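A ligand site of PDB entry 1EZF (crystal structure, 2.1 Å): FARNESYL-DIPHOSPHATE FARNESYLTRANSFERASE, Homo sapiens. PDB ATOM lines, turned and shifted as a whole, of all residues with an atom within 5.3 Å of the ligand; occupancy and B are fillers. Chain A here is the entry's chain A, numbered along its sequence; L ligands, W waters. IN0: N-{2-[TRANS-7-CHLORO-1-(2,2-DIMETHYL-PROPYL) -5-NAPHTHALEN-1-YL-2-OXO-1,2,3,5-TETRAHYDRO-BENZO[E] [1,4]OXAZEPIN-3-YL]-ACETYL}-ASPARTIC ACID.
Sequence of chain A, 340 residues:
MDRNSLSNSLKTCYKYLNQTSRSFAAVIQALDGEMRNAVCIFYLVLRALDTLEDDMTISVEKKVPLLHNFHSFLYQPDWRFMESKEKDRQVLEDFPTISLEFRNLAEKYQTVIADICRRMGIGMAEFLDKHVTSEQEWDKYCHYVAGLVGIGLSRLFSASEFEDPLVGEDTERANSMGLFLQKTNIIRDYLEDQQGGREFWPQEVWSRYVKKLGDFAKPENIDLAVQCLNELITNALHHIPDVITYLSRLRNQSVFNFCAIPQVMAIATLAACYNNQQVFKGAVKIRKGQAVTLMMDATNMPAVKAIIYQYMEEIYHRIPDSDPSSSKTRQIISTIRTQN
An oxygen (O64) of the ligand lies within salt-bridge range of the guanidinium group (NE) of Arg 22 (3.1 Å). The side-chain hydroxyl (OG) of Ser 23 lies within hydrogen-bond range of an oxygen (O65) of the ligand (3.3 Å).
The side-chain hydroxyl (OH) of Tyr 43 is in hydrogen-bond range of the side-chain hydroxyl (OG) of Ser 21, at 3.2 Å. The side-chain hydroxyl (OH) of Tyr 43 sits at hydrogen-bond distance from the backbone carbonyl oxygen (O) of Thr 20 (3.2 Å). The side-chain amide nitrogen (ND2) of Asn 185 lies within hydrogen-bond range of the backbone carbonyl oxygen (O) of Leu 181. The backbone carbonyl oxygen of Met 177 is in hydrogen-bond range of the side-chain amide nitrogen of Gln 263, 3.1 Å away. OD1 of Asn 185 is in hydrogen-bond range of NH2 of Arg 188.
Phe 24 touches the ligand (CD2 to O58, 3.5 Å). Phe 42 touches the ligand. Tyr 43 touches the ligand (CD2 to C9, 3.4 Å). CD1 of Leu 46 touches C9 of the ligand, at 3.8 Å. Ala 146 touches the ligand (O to C31, 3.4 Å). Val 149 touches the ligand. Gly 150 touches the ligand (CA to C30, 3.2 Å). Leu 153 touches the ligand (CD1 to C16, 3.6 Å). Met 177 touches the ligand. Gly 178 touches the ligand. Leu 181 touches the ligand. Gln 182 touches the ligand (OE1 to C25, 3.0 Å). ND2 of Asn 185 touches C32 of the ligand, at 3.996 Å. Phe 258 touches the ligand (CE2 to C27, 3.6 Å). CA of Cys 259 touches C27 of the ligand, at 3.9 Å. CG of Pro 262 touches O6 of the ligand (3.7 Å). Met 265 touches the ligand (CE to O66, 3.9 Å). Within 4 Å of the ligand: Arg 22, Ser 23, Phe 24, Phe 42, Tyr 43, Leu 46, Ala 146, Val 149, Gly 150, Leu 153, Met 177, Gly 178, Leu 181, Gln 182, Asn 185, Phe 258, Cys 259, Pro 262 and Met 265. The nearest printed residue that does not touch the ligand is Val 145 (4.1 Å).
Water W2 bridges the backbone carbonyl oxygen of Cys 259 (2.8 Å) and the side-chain amide nitrogen of Gln 263 (2.9 Å). Water W3 bridges the side-chain sulfur of Met 265 (3.1 Å) and a nitrogen (N23) of the ligand (3.3 Å).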
ATOM      1  N   THR A  20      22.421   8.003  27.574  1.00  0.00           N
ATOM      2  CA  THR A  20      23.516   7.232  26.969  1.00  0.00           C
ATOM      3  C   THR A  20      23.002   6.129  26.061  1.00  0.00           C
ATOM      4  O   THR A  20      23.783   5.453  25.378  1.00  0.00           O
ATOM      5  CB  THR A  20      24.433   6.605  28.040  1.00  0.00           C
ATOM      6  OG1 THR A  20      23.713   5.631  28.790  1.00  0.00           O
ATOM      7  CG2 THR A  20      24.961   7.679  28.980  1.00  0.00           C
ATOM      8  N   SER A  21      21.690   5.914  26.059  1.00  0.00           N
ATOM      9  CA  SER A  21      21.086   4.880  25.232  1.00  0.00           C
ATOM     10  C   SER A  21      19.953   5.491  24.424  1.00  0.00           C
ATOM     11  O   SER A  21      19.047   6.119  24.958  1.00  0.00           O
ATOM     12  CB  SER A  21      20.582   3.730  26.097  1.00  0.00           C
ATOM     13  OG  SER A  21      20.618   2.507  25.382  1.00  0.00           O
ATOM     14  N   ARG A  22      20.030   5.310  23.115  1.00  0.00           N
ATOM     15  CA  ARG A  22      19.024   5.852  22.205  1.00  0.00           C
ATOM     16  C   ARG A  22      17.726   5.065  22.183  1.00  0.00           C
ATOM     17  O   ARG A  22      16.647   5.633  22.070  1.00  0.00           O
ATOM     18  CB  ARG A  22      19.591   5.917  20.786  1.00  0.00           C
ATOM     19  CG  ARG A  22      19.958   4.555  20.219  1.00  0.00           C
ATOM     20  CD  ARG A  22      20.509   4.656  18.812  1.00  0.00           C
ATOM     21  NE  ARG A  22      21.863   5.228  18.781  1.00  0.00           N
ATOM     22  CZ  ARG A  22      22.378   5.845  17.736  1.00  0.00           C
ATOM     23  NH1 ARG A  22      21.671   5.973  16.613  1.00  0.00           N
ATOM     24  NH2 ARG A  22      23.610   6.336  17.791  1.00  0.00           N
ATOM     25  N   SER A  23      17.833   3.739  22.271  1.00  0.00           N
ATOM     26  CA  SER A  23      16.649   2.890  22.226  1.00  0.00           C
ATOM     27  C   SER A  23      16.670   1.740  23.212  1.00  0.00           C
ATOM     28  O   SER A  23      15.614   1.278  23.659  1.00  0.00           O
ATOM     29  CB  SER A  23      16.482   2.335  20.808  1.00  0.00           C
ATOM     30  OG  SER A  23      17.719   1.843  20.316  1.00  0.00           O
ATOM     31  N   PHE A  24      17.866   1.302  23.579  1.00  0.00           N
ATOM     32  CA  PHE A  24      18.005   0.175  24.478  1.00  0.00           C
ATOM     33  C   PHE A  24      17.576   0.418  25.933  1.00  0.00           C
ATOM     34  O   PHE A  24      17.361  -0.543  26.674  1.00  0.00           O
ATOM     35  CB  PHE A  24      19.428  -0.369  24.413  1.00  0.00           C
ATOM     36  CG  PHE A  24      19.526  -1.823  24.749  1.00  0.00           C
ATOM     37  CD1 PHE A  24      18.748  -2.760  24.063  1.00  0.00           C
ATOM     38  CD2 PHE A  24      20.380  -2.268  25.751  1.00  0.00           C
ATOM     39  CE1 PHE A  24      18.812  -4.111  24.378  1.00  0.00           C
ATOM     40  CE2 PHE A  24      20.454  -3.614  26.075  1.00  0.00           C
ATOM     41  CZ  PHE A  24      19.668  -4.542  25.383  1.00  0.00           C
ATOM     42  N   VAL A  39      20.837  -4.129  36.179  1.00  0.00           N
ATOM     43  CA  VAL A  39      21.326  -3.948  34.818  1.00  0.00           C
ATOM     44  C   VAL A  39      21.434  -2.464  34.447  1.00  0.00           C
ATOM     45  O   VAL A  39      22.310  -2.094  33.666  1.00  0.00           O
ATOM     46  CB  VAL A  39      20.467  -4.703  33.782  1.00  0.00           C
ATOM     47  CG1 VAL A  39      20.863  -4.320  32.343  1.00  0.00           C
ATOM     48  CG2 VAL A  39      20.641  -6.213  33.980  1.00  0.00           C
ATOM     49  N   PHE A  42      24.687  -1.464  36.022  1.00  0.00           N
ATOM     50  CA  PHE A  42      25.749  -2.155  35.296  1.00  0.00           C
ATOM     51  C   PHE A  42      26.101  -1.437  33.999  1.00  0.00           C
ATOM     52  O   PHE A  42      27.277  -1.208  33.690  1.00  0.00           O
ATOM     53  CB  PHE A  42      25.330  -3.598  34.973  1.00  0.00           C
ATOM     54  CG  PHE A  42      26.467  -4.499  34.560  1.00  0.00           C
ATOM     55  CD1 PHE A  42      27.769  -4.238  34.998  1.00  0.00           C
ATOM     56  CD2 PHE A  42      26.235  -5.621  33.776  1.00  0.00           C
ATOM     57  CE1 PHE A  42      28.826  -5.083  34.650  1.00  0.00           C
ATOM     58  CE2 PHE A  42      27.278  -6.465  33.432  1.00  0.00           C
ATOM     59  CZ  PHE A  42      28.571  -6.209  33.862  1.00  0.00           C
ATOM     60  N   TYR A  43      25.067  -1.087  33.232  1.00  0.00           N
ATOM     61  CA  TYR A  43      25.226  -0.401  31.966  1.00  0.00           C
ATOM     62  C   TYR A  43      25.899   0.960  32.164  1.00  0.00           C
ATOM     63  O   TYR A  43      26.851   1.290  31.459  1.00  0.00           O
ATOM     64  CB  TYR A  43      23.849  -0.255  31.291  1.00  0.00           C
ATOM     65  CG  TYR A  43      23.849   0.413  29.934  1.00  0.00           C
ATOM     66  CD1 TYR A  43      23.981   1.808  29.812  1.00  0.00           C
ATOM     67  CD2 TYR A  43      23.695  -0.329  28.754  1.00  0.00           C
ATOM     68  CE1 TYR A  43      23.947   2.434  28.581  1.00  0.00           C
ATOM     69  CE2 TYR A  43      23.648   0.295  27.505  1.00  0.00           C
ATOM     70  CZ  TYR A  43      23.778   1.680  27.433  1.00  0.00           C
ATOM     71  OH  TYR A  43      23.726   2.329  26.212  1.00  0.00           O
ATOM     72  N   LEU A  46      29.592   0.494  33.202  1.00  0.00           N
ATOM     73  CA  LEU A  46      30.346   0.050  32.029  1.00  0.00           C
ATOM     74  C   LEU A  46      30.484   1.195  31.034  1.00  0.00           C
ATOM     75  O   LEU A  46      31.442   1.260  30.266  1.00  0.00           O
ATOM     76  CB  LEU A  46      29.652  -1.133  31.349  1.00  0.00           C
ATOM     77  CG  LEU A  46      29.733  -2.509  32.004  1.00  0.00           C
ATOM     78  CD1 LEU A  46      28.793  -3.456  31.293  1.00  0.00           C
ATOM     79  CD2 LEU A  46      31.159  -3.055  31.949  1.00  0.00           C
ATOM     80  N   ASP A  50      33.991   2.780  29.697  1.00  0.00           N
ATOM     81  CA  ASP A  50      34.139   2.834  28.255  1.00  0.00           C
ATOM     82  C   ASP A  50      34.512   4.241  27.800  1.00  0.00           C
ATOM     83  O   ASP A  50      35.408   4.424  26.959  1.00  0.00           O
ATOM     84  CB  ASP A  50      32.843   2.389  27.571  1.00  0.00           C
ATOM     85  CG  ASP A  50      32.560   0.898  27.763  1.00  0.00           C
ATOM     86  OD1 ASP A  50      33.410   0.172  28.320  1.00  0.00           O
ATOM     87  OD2 ASP A  50      31.478   0.450  27.352  1.00  0.00           O
ATOM     88  N   VAL A 145      36.380  -6.449  26.929  1.00  0.00           N
ATOM     89  CA  VAL A 145      35.401  -5.362  26.922  1.00  0.00           C
ATOM     90  C   VAL A 145      33.937  -5.715  26.619  1.00  0.00           C
ATOM     91  O   VAL A 145      33.040  -4.902  26.834  1.00  0.00           O
ATOM     92  CB  VAL A 145      35.877  -4.215  25.978  1.00  0.00           C
ATOM     93  CG1 VAL A 145      37.294  -3.799  26.360  1.00  0.00           C
ATOM     94  CG2 VAL A 145      35.816  -4.650  24.539  1.00  0.00           C
ATOM     95  N   ALA A 146      33.684  -6.931  26.137  1.00  0.00           N
ATOM     96  CA  ALA A 146      32.335  -7.316  25.808  1.00  0.00           C
ATOM     97  C   ALA A 146      32.034  -8.729  26.286  1.00  0.00           C
ATOM     98  O   ALA A 146      30.921  -9.009  26.736  1.00  0.00           O
ATOM     99  CB  ALA A 146      32.099  -7.191  24.311  1.00  0.00           C
ATOM    100  N   GLY A 147      33.024  -9.615  26.189  1.00  0.00           N
ATOM    101  CA  GLY A 147      32.831 -10.988  26.649  1.00  0.00           C
ATOM    102  C   GLY A 147      32.493 -10.981  28.132  1.00  0.00           C
ATOM    103  O   GLY A 147      31.490 -11.555  28.560  1.00  0.00           O
ATOM    104  N   VAL A 149      31.251  -8.714  29.798  1.00  0.00           N
ATOM    105  CA  VAL A 149      29.933  -8.097  30.011  1.00  0.00           C
ATOM    106  C   VAL A 149      28.874  -9.199  29.908  1.00  0.00           C
ATOM    107  O   VAL A 149      27.914  -9.229  30.684  1.00  0.00           O
ATOM    108  CB  VAL A 149      29.671  -6.972  28.985  1.00  0.00           C
ATOM    109  CG1 VAL A 149      28.266  -6.394  29.159  1.00  0.00           C
ATOM    110  CG2 VAL A 149      30.703  -5.865  29.149  1.00  0.00           C
ATOM    111  N   GLY A 150      29.075 -10.121  28.955  1.00  0.00           N
ATOM    112  CA  GLY A 150      28.159 -11.228  28.783  1.00  0.00           C
ATOM    113  C   GLY A 150      28.250 -12.114  30.003  1.00  0.00           C
ATOM    114  O   GLY A 150      27.230 -12.564  30.549  1.00  0.00           O
ATOM    115  N   LEU A 153      26.496 -10.226  32.980  1.00  0.00           N
ATOM    116  CA  LEU A 153      25.047 -10.269  32.830  1.00  0.00           C
ATOM    117  C   LEU A 153      24.539 -11.662  33.164  1.00  0.00           C
ATOM    118  O   LEU A 153      23.680 -11.795  34.018  1.00  0.00           O
ATOM    119  CB  LEU A 153      24.629  -9.852  31.415  1.00  0.00           C
ATOM    120  CG  LEU A 153      24.738  -8.348  31.123  1.00  0.00           C
ATOM    121  CD1 LEU A 153      24.669  -8.095  29.634  1.00  0.00           C
ATOM    122  CD2 LEU A 153      23.638  -7.578  31.845  1.00  0.00           C
ATOM    123  N   ALA A 174      28.350 -17.186  27.194  1.00  0.00           N
ATOM    124  CA  ALA A 174      28.159 -15.772  27.528  1.00  0.00           C
ATOM    125  C   ALA A 174      29.241 -14.916  26.870  1.00  0.00           C
ATOM    126  O   ALA A 174      28.971 -13.817  26.390  1.00  0.00           O
ATOM    127  CB  ALA A 174      28.181 -15.586  29.035  1.00  0.00           C
ATOM    128  N   MET A 177      28.627 -14.364  23.104  1.00  0.00           N
ATOM    129  CA  MET A 177      27.592 -13.351  22.915  1.00  0.00           C
ATOM    130  C   MET A 177      28.287 -11.994  22.820  1.00  0.00           C
ATOM    131  O   MET A 177      28.040 -11.228  21.876  1.00  0.00           O
ATOM    132  CB  MET A 177      26.631 -13.348  24.111  1.00  0.00           C
ATOM    133  CG  MET A 177      25.625 -14.517  24.168  1.00  0.00           C
ATOM    134  SD  MET A 177      24.191 -14.337  23.062  1.00  0.00           S
ATOM    135  CE  MET A 177      23.344 -12.973  23.805  1.00  0.00           C
ATOM    136  N   GLY A 178      29.177 -11.727  23.767  1.00  0.00           N
ATOM    137  CA  GLY A 178      29.906 -10.465  23.800  1.00  0.00           C
ATOM    138  C   GLY A 178      30.841 -10.244  22.631  1.00  0.00           C
ATOM    139  O   GLY A 178      30.900  -9.142  22.089  1.00  0.00           O
ATOM    140  N   LEU A 181      28.886  -9.167  19.401  1.00  0.00           N
ATOM    141  CA  LEU A 181      28.534  -7.756  19.384  1.00  0.00           C
ATOM    142  C   LEU A 181      29.755  -6.842  19.223  1.00  0.00           C
ATOM    143  O   LEU A 181      29.738  -5.903  18.420  1.00  0.00           O
ATOM    144  CB  LEU A 181      27.802  -7.363  20.655  1.00  0.00           C
ATOM    145  CG  LEU A 181      26.492  -8.073  21.024  1.00  0.00           C
ATOM    146  CD1 LEU A 181      25.947  -7.449  22.290  1.00  0.00           C
ATOM    147  CD2 LEU A 181      25.480  -7.952  19.892  1.00  0.00           C
ATOM    148  N   GLN A 182      30.805  -7.101  19.996  1.00  0.00           N
ATOM    149  CA  GLN A 182      32.002  -6.274  19.959  1.00  0.00           C
ATOM    150  C   GLN A 182      32.672  -6.235  18.603  1.00  0.00           C
ATOM    151  O   GLN A 182      33.047  -5.165  18.121  1.00  0.00           O
ATOM    152  CB  GLN A 182      33.002  -6.719  21.008  1.00  0.00           C
ATOM    153  CG  GLN A 182      34.055  -5.660  21.293  1.00  0.00           C
ATOM    154  CD  GLN A 182      33.423  -4.350  21.684  1.00  0.00           C
ATOM    155  OE1 GLN A 182      32.734  -4.267  22.692  1.00  0.00           O
ATOM    156  NE2 GLN A 182      33.595  -3.329  20.851  1.00  0.00           N
ATOM    157  N   ASN A 185      30.739  -4.214  16.030  1.00  0.00           N
ATOM    158  CA  ASN A 185      30.906  -2.785  16.298  1.00  0.00           C
ATOM    159  C   ASN A 185      32.286  -2.262  15.837  1.00  0.00           C
ATOM    160  O   ASN A 185      32.378  -1.206  15.213  1.00  0.00           O
ATOM    161  CB  ASN A 185      30.711  -2.477  17.783  1.00  0.00           C
ATOM    162  CG  ASN A 185      29.283  -2.672  18.238  1.00  0.00           C
ATOM    163  OD1 ASN A 185      28.336  -2.411  17.492  1.00  0.00           O
ATOM    164  ND2 ASN A 185      29.122  -3.172  19.442  1.00  0.00           N
ATOM    165  N   ARG A 188      32.117  -2.196  12.014  1.00  0.00           N
ATOM    166  CA  ARG A 188      31.250  -1.092  11.581  1.00  0.00           C
ATOM    167  C   ARG A 188      31.844   0.277  11.864  1.00  0.00           C
ATOM    168  O   ARG A 188      31.768   1.174  11.023  1.00  0.00           O
ATOM    169  CB  ARG A 188      29.883  -1.201  12.262  1.00  0.00           C
ATOM    170  CG  ARG A 188      28.906  -0.081  11.903  1.00  0.00           C
ATOM    171  CD  ARG A 188      28.542   0.760  13.121  1.00  0.00           C
ATOM    172  NE  ARG A 188      27.609   0.072  14.002  1.00  0.00           N
ATOM    173  CZ  ARG A 188      27.618   0.180  15.325  1.00  0.00           C
ATOM    174  NH1 ARG A 188      28.502   0.934  15.942  1.00  0.00           N
ATOM    175  NH2 ARG A 188      26.697  -0.456  16.046  1.00  0.00           N
ATOM    176  N   PHE A 258      15.902  -8.771  26.076  1.00  0.00           N
ATOM    177  CA  PHE A 258      17.100  -8.011  26.413  1.00  0.00           C
ATOM    178  C   PHE A 258      18.322  -8.523  25.625  1.00  0.00           C
ATOM    179  O   PHE A 258      19.019  -7.751  24.961  1.00  0.00           O
ATOM    180  CB  PHE A 258      17.343  -8.110  27.926  1.00  0.00           C
ATOM    181  CG  PHE A 258      18.557  -7.375  28.412  1.00  0.00           C
ATOM    182  CD1 PHE A 258      18.608  -5.985  28.373  1.00  0.00           C
ATOM    183  CD2 PHE A 258      19.660  -8.070  28.891  1.00  0.00           C
ATOM    184  CE1 PHE A 258      19.734  -5.302  28.817  1.00  0.00           C
ATOM    185  CE2 PHE A 258      20.786  -7.387  29.335  1.00  0.00           C
ATOM    186  CZ  PHE A 258      20.829  -6.003  29.296  1.00  0.00           C
ATOM    187  N   CYS A 259      18.530  -9.835  25.649  1.00  0.00           N
ATOM    188  CA  CYS A 259      19.664 -10.422  24.971  1.00  0.00           C
ATOM    189  C   CYS A 259      19.512 -10.576  23.462  1.00  0.00           C
ATOM    190  O   CYS A 259      20.455 -10.331  22.719  1.00  0.00           O
ATOM    191  CB  CYS A 259      19.985 -11.794  25.586  1.00  0.00           C
ATOM    192  SG  CYS A 259      20.413 -11.752  27.359  1.00  0.00           S
ATOM    193  N   PRO A 262      19.992  -7.072  20.748  1.00  0.00           N
ATOM    194  CA  PRO A 262      21.329  -6.690  20.254  1.00  0.00           C
ATOM    195  C   PRO A 262      21.936  -7.698  19.274  1.00  0.00           C
ATOM    196  O   PRO A 262      22.565  -7.312  18.284  1.00  0.00           O
ATOM    197  CB  PRO A 262      22.147  -6.592  21.550  1.00  0.00           C
ATOM    198  CG  PRO A 262      21.144  -6.111  22.529  1.00  0.00           C
ATOM    199  CD  PRO A 262      19.969  -7.024  22.214  1.00  0.00           C
ATOM    200  N   GLN A 263      21.729  -8.992  19.523  1.00  0.00           N
ATOM    201  CA  GLN A 263      22.276 -10.029  18.657  1.00  0.00           C
ATOM    202  C   GLN A 263      21.628 -10.010  17.272  1.00  0.00           C
ATOM    203  O   GLN A 263      22.288 -10.325  16.281  1.00  0.00           O
ATOM    204  CB  GLN A 263      22.138 -11.409  19.292  1.00  0.00           C
ATOM    205  CG  GLN A 263      22.818 -11.549  20.642  1.00  0.00           C
ATOM    206  CD  GLN A 263      24.351 -11.501  20.560  1.00  0.00           C
ATOM    207  OE1 GLN A 263      24.951 -11.824  19.540  1.00  0.00           O
ATOM    208  NE2 GLN A 263      24.986 -11.084  21.659  1.00  0.00           N
ATOM    209  N   MET A 265      20.281  -7.220  15.892  1.00  0.00           N
ATOM    210  CA  MET A 265      20.718  -5.948  15.336  1.00  0.00           C
ATOM    211  C   MET A 265      22.160  -6.089  14.843  1.00  0.00           C
ATOM    212  O   MET A 265      22.544  -5.466  13.853  1.00  0.00           O
ATOM    213  CB  MET A 265      20.632  -4.858  16.393  1.00  0.00           C
ATOM    214  CG  MET A 265      19.212  -4.482  16.788  1.00  0.00           C
ATOM    215  SD  MET A 265      19.207  -3.177  18.023  1.00  0.00           S
ATOM    216  CE  MET A 265      19.190  -1.704  16.984  1.00  0.00           C
HETATM  217  C1  IN0 L   1      25.294  -4.417  26.564  1.00  0.00           C
HETATM  218  C7  IN0 L   1      24.839  -5.328  25.411  1.00  0.00           C
HETATM  219  C17 IN0 L   1      24.413  -6.752  25.812  1.00  0.00           C
HETATM  220  C28 IN0 L   1      23.058  -7.053  26.055  1.00  0.00           C
HETATM  221  C27 IN0 L   1      22.658  -8.358  26.382  1.00  0.00           C
HETATM  222  C26 IN0 L   1      23.628  -9.379  26.470  1.00  0.00           C
HETATM  223  C16 IN0 L   1      24.990  -9.102  26.231  1.00  0.00           C
HETATM  224  C29 IN0 L   1      25.956 -10.122  26.278  1.00  0.00           C
HETATM  225  C30 IN0 L   1      27.305  -9.847  26.021  1.00  0.00           C
HETATM  226  C31 IN0 L   1      27.701  -8.537  25.706  1.00  0.00           C
HETATM  227  C33 IN0 L   1      26.751  -7.504  25.658  1.00  0.00           C
HETATM  228  C15 IN0 L   1      25.391  -7.783  25.907  1.00  0.00           C
HETATM  229  O6  IN0 L   1      23.827  -4.690  24.610  1.00  0.00           O
HETATM  230  C5  IN0 L   1      24.131  -3.320  24.238  1.00  0.00           C
HETATM  231  C14 IN0 L   1      23.175  -2.905  23.086  1.00  0.00           C
HETATM  232  C11 IN0 L   1      23.035  -1.417  22.938  1.00  0.00           C
HETATM  233  O58 IN0 L   1      22.953  -0.716  23.936  1.00  0.00           O
HETATM  234  N23 IN0 L   1      23.013  -0.903  21.677  1.00  0.00           N
HETATM  235  C38 IN0 L   1      22.885   0.550  21.476  1.00  0.00           C
HETATM  236  C61 IN0 L   1      24.094   1.148  20.716  1.00  0.00           C
HETATM  237  C62 IN0 L   1      23.820   2.589  20.305  1.00  0.00           C
HETATM  238  O64 IN0 L   1      23.788   2.826  18.983  1.00  0.00           O
HETATM  239  O63 IN0 L   1      23.639   3.476  21.128  1.00  0.00           O
HETATM  240  C60 IN0 L   1      21.606   0.871  20.733  1.00  0.00           C
HETATM  241  O66 IN0 L   1      21.302   0.161  19.641  1.00  0.00           O
HETATM  242  O65 IN0 L   1      20.877   1.762  21.135  1.00  0.00           O
HETATM  243  C4  IN0 L   1      25.594  -3.143  23.887  1.00  0.00           C
HETATM  244  O13 IN0 L   1      25.894  -3.081  22.704  1.00  0.00           O
HETATM  245  N3  IN0 L   1      26.519  -3.056  24.909  1.00  0.00           N
HETATM  246  C2  IN0 L   1      26.128  -3.309  26.272  1.00  0.00           C
HETATM  247  C8  IN0 L   1      26.575  -2.478  27.313  1.00  0.00           C
HETATM  248  C9  IN0 L   1      26.169  -2.717  28.619  1.00  0.00           C
HETATM  249  C20 IN0 L   1      25.315  -3.801  28.912  1.00  0.00           C
HETATM  250 CL36 IN0 L   1      24.790  -4.075  30.547  1.00  0.00          CL
HETATM  251  C21 IN0 L   1      24.884  -4.652  27.883  1.00  0.00           C
HETATM  252  C43 IN0 L   1      27.900  -2.633  24.615  1.00  0.00           C
HETATM  253  C10 IN0 L   1      29.009  -3.706  24.391  1.00  0.00           C
HETATM  254  C32 IN0 L   1      28.671  -4.593  23.150  1.00  0.00           C
HETATM  255  C25 IN0 L   1      30.395  -3.016  24.147  1.00  0.00           C
HETATM  256  C24 IN0 L   1      29.145  -4.645  25.630  1.00  0.00           C
HETATM  257  O   HOH W   1      33.293  -1.729  24.440  1.00  0.00           O
HETATM  258  O   HOH W   2      23.066  -9.607  23.261  1.00  0.00           O
HETATM  259  O   HOH W   3      21.695  -3.351  19.921  1.00  0.00           O
HETATM  260  O   HOH W   4      25.748  -3.901  20.256  1.00  0.00           O
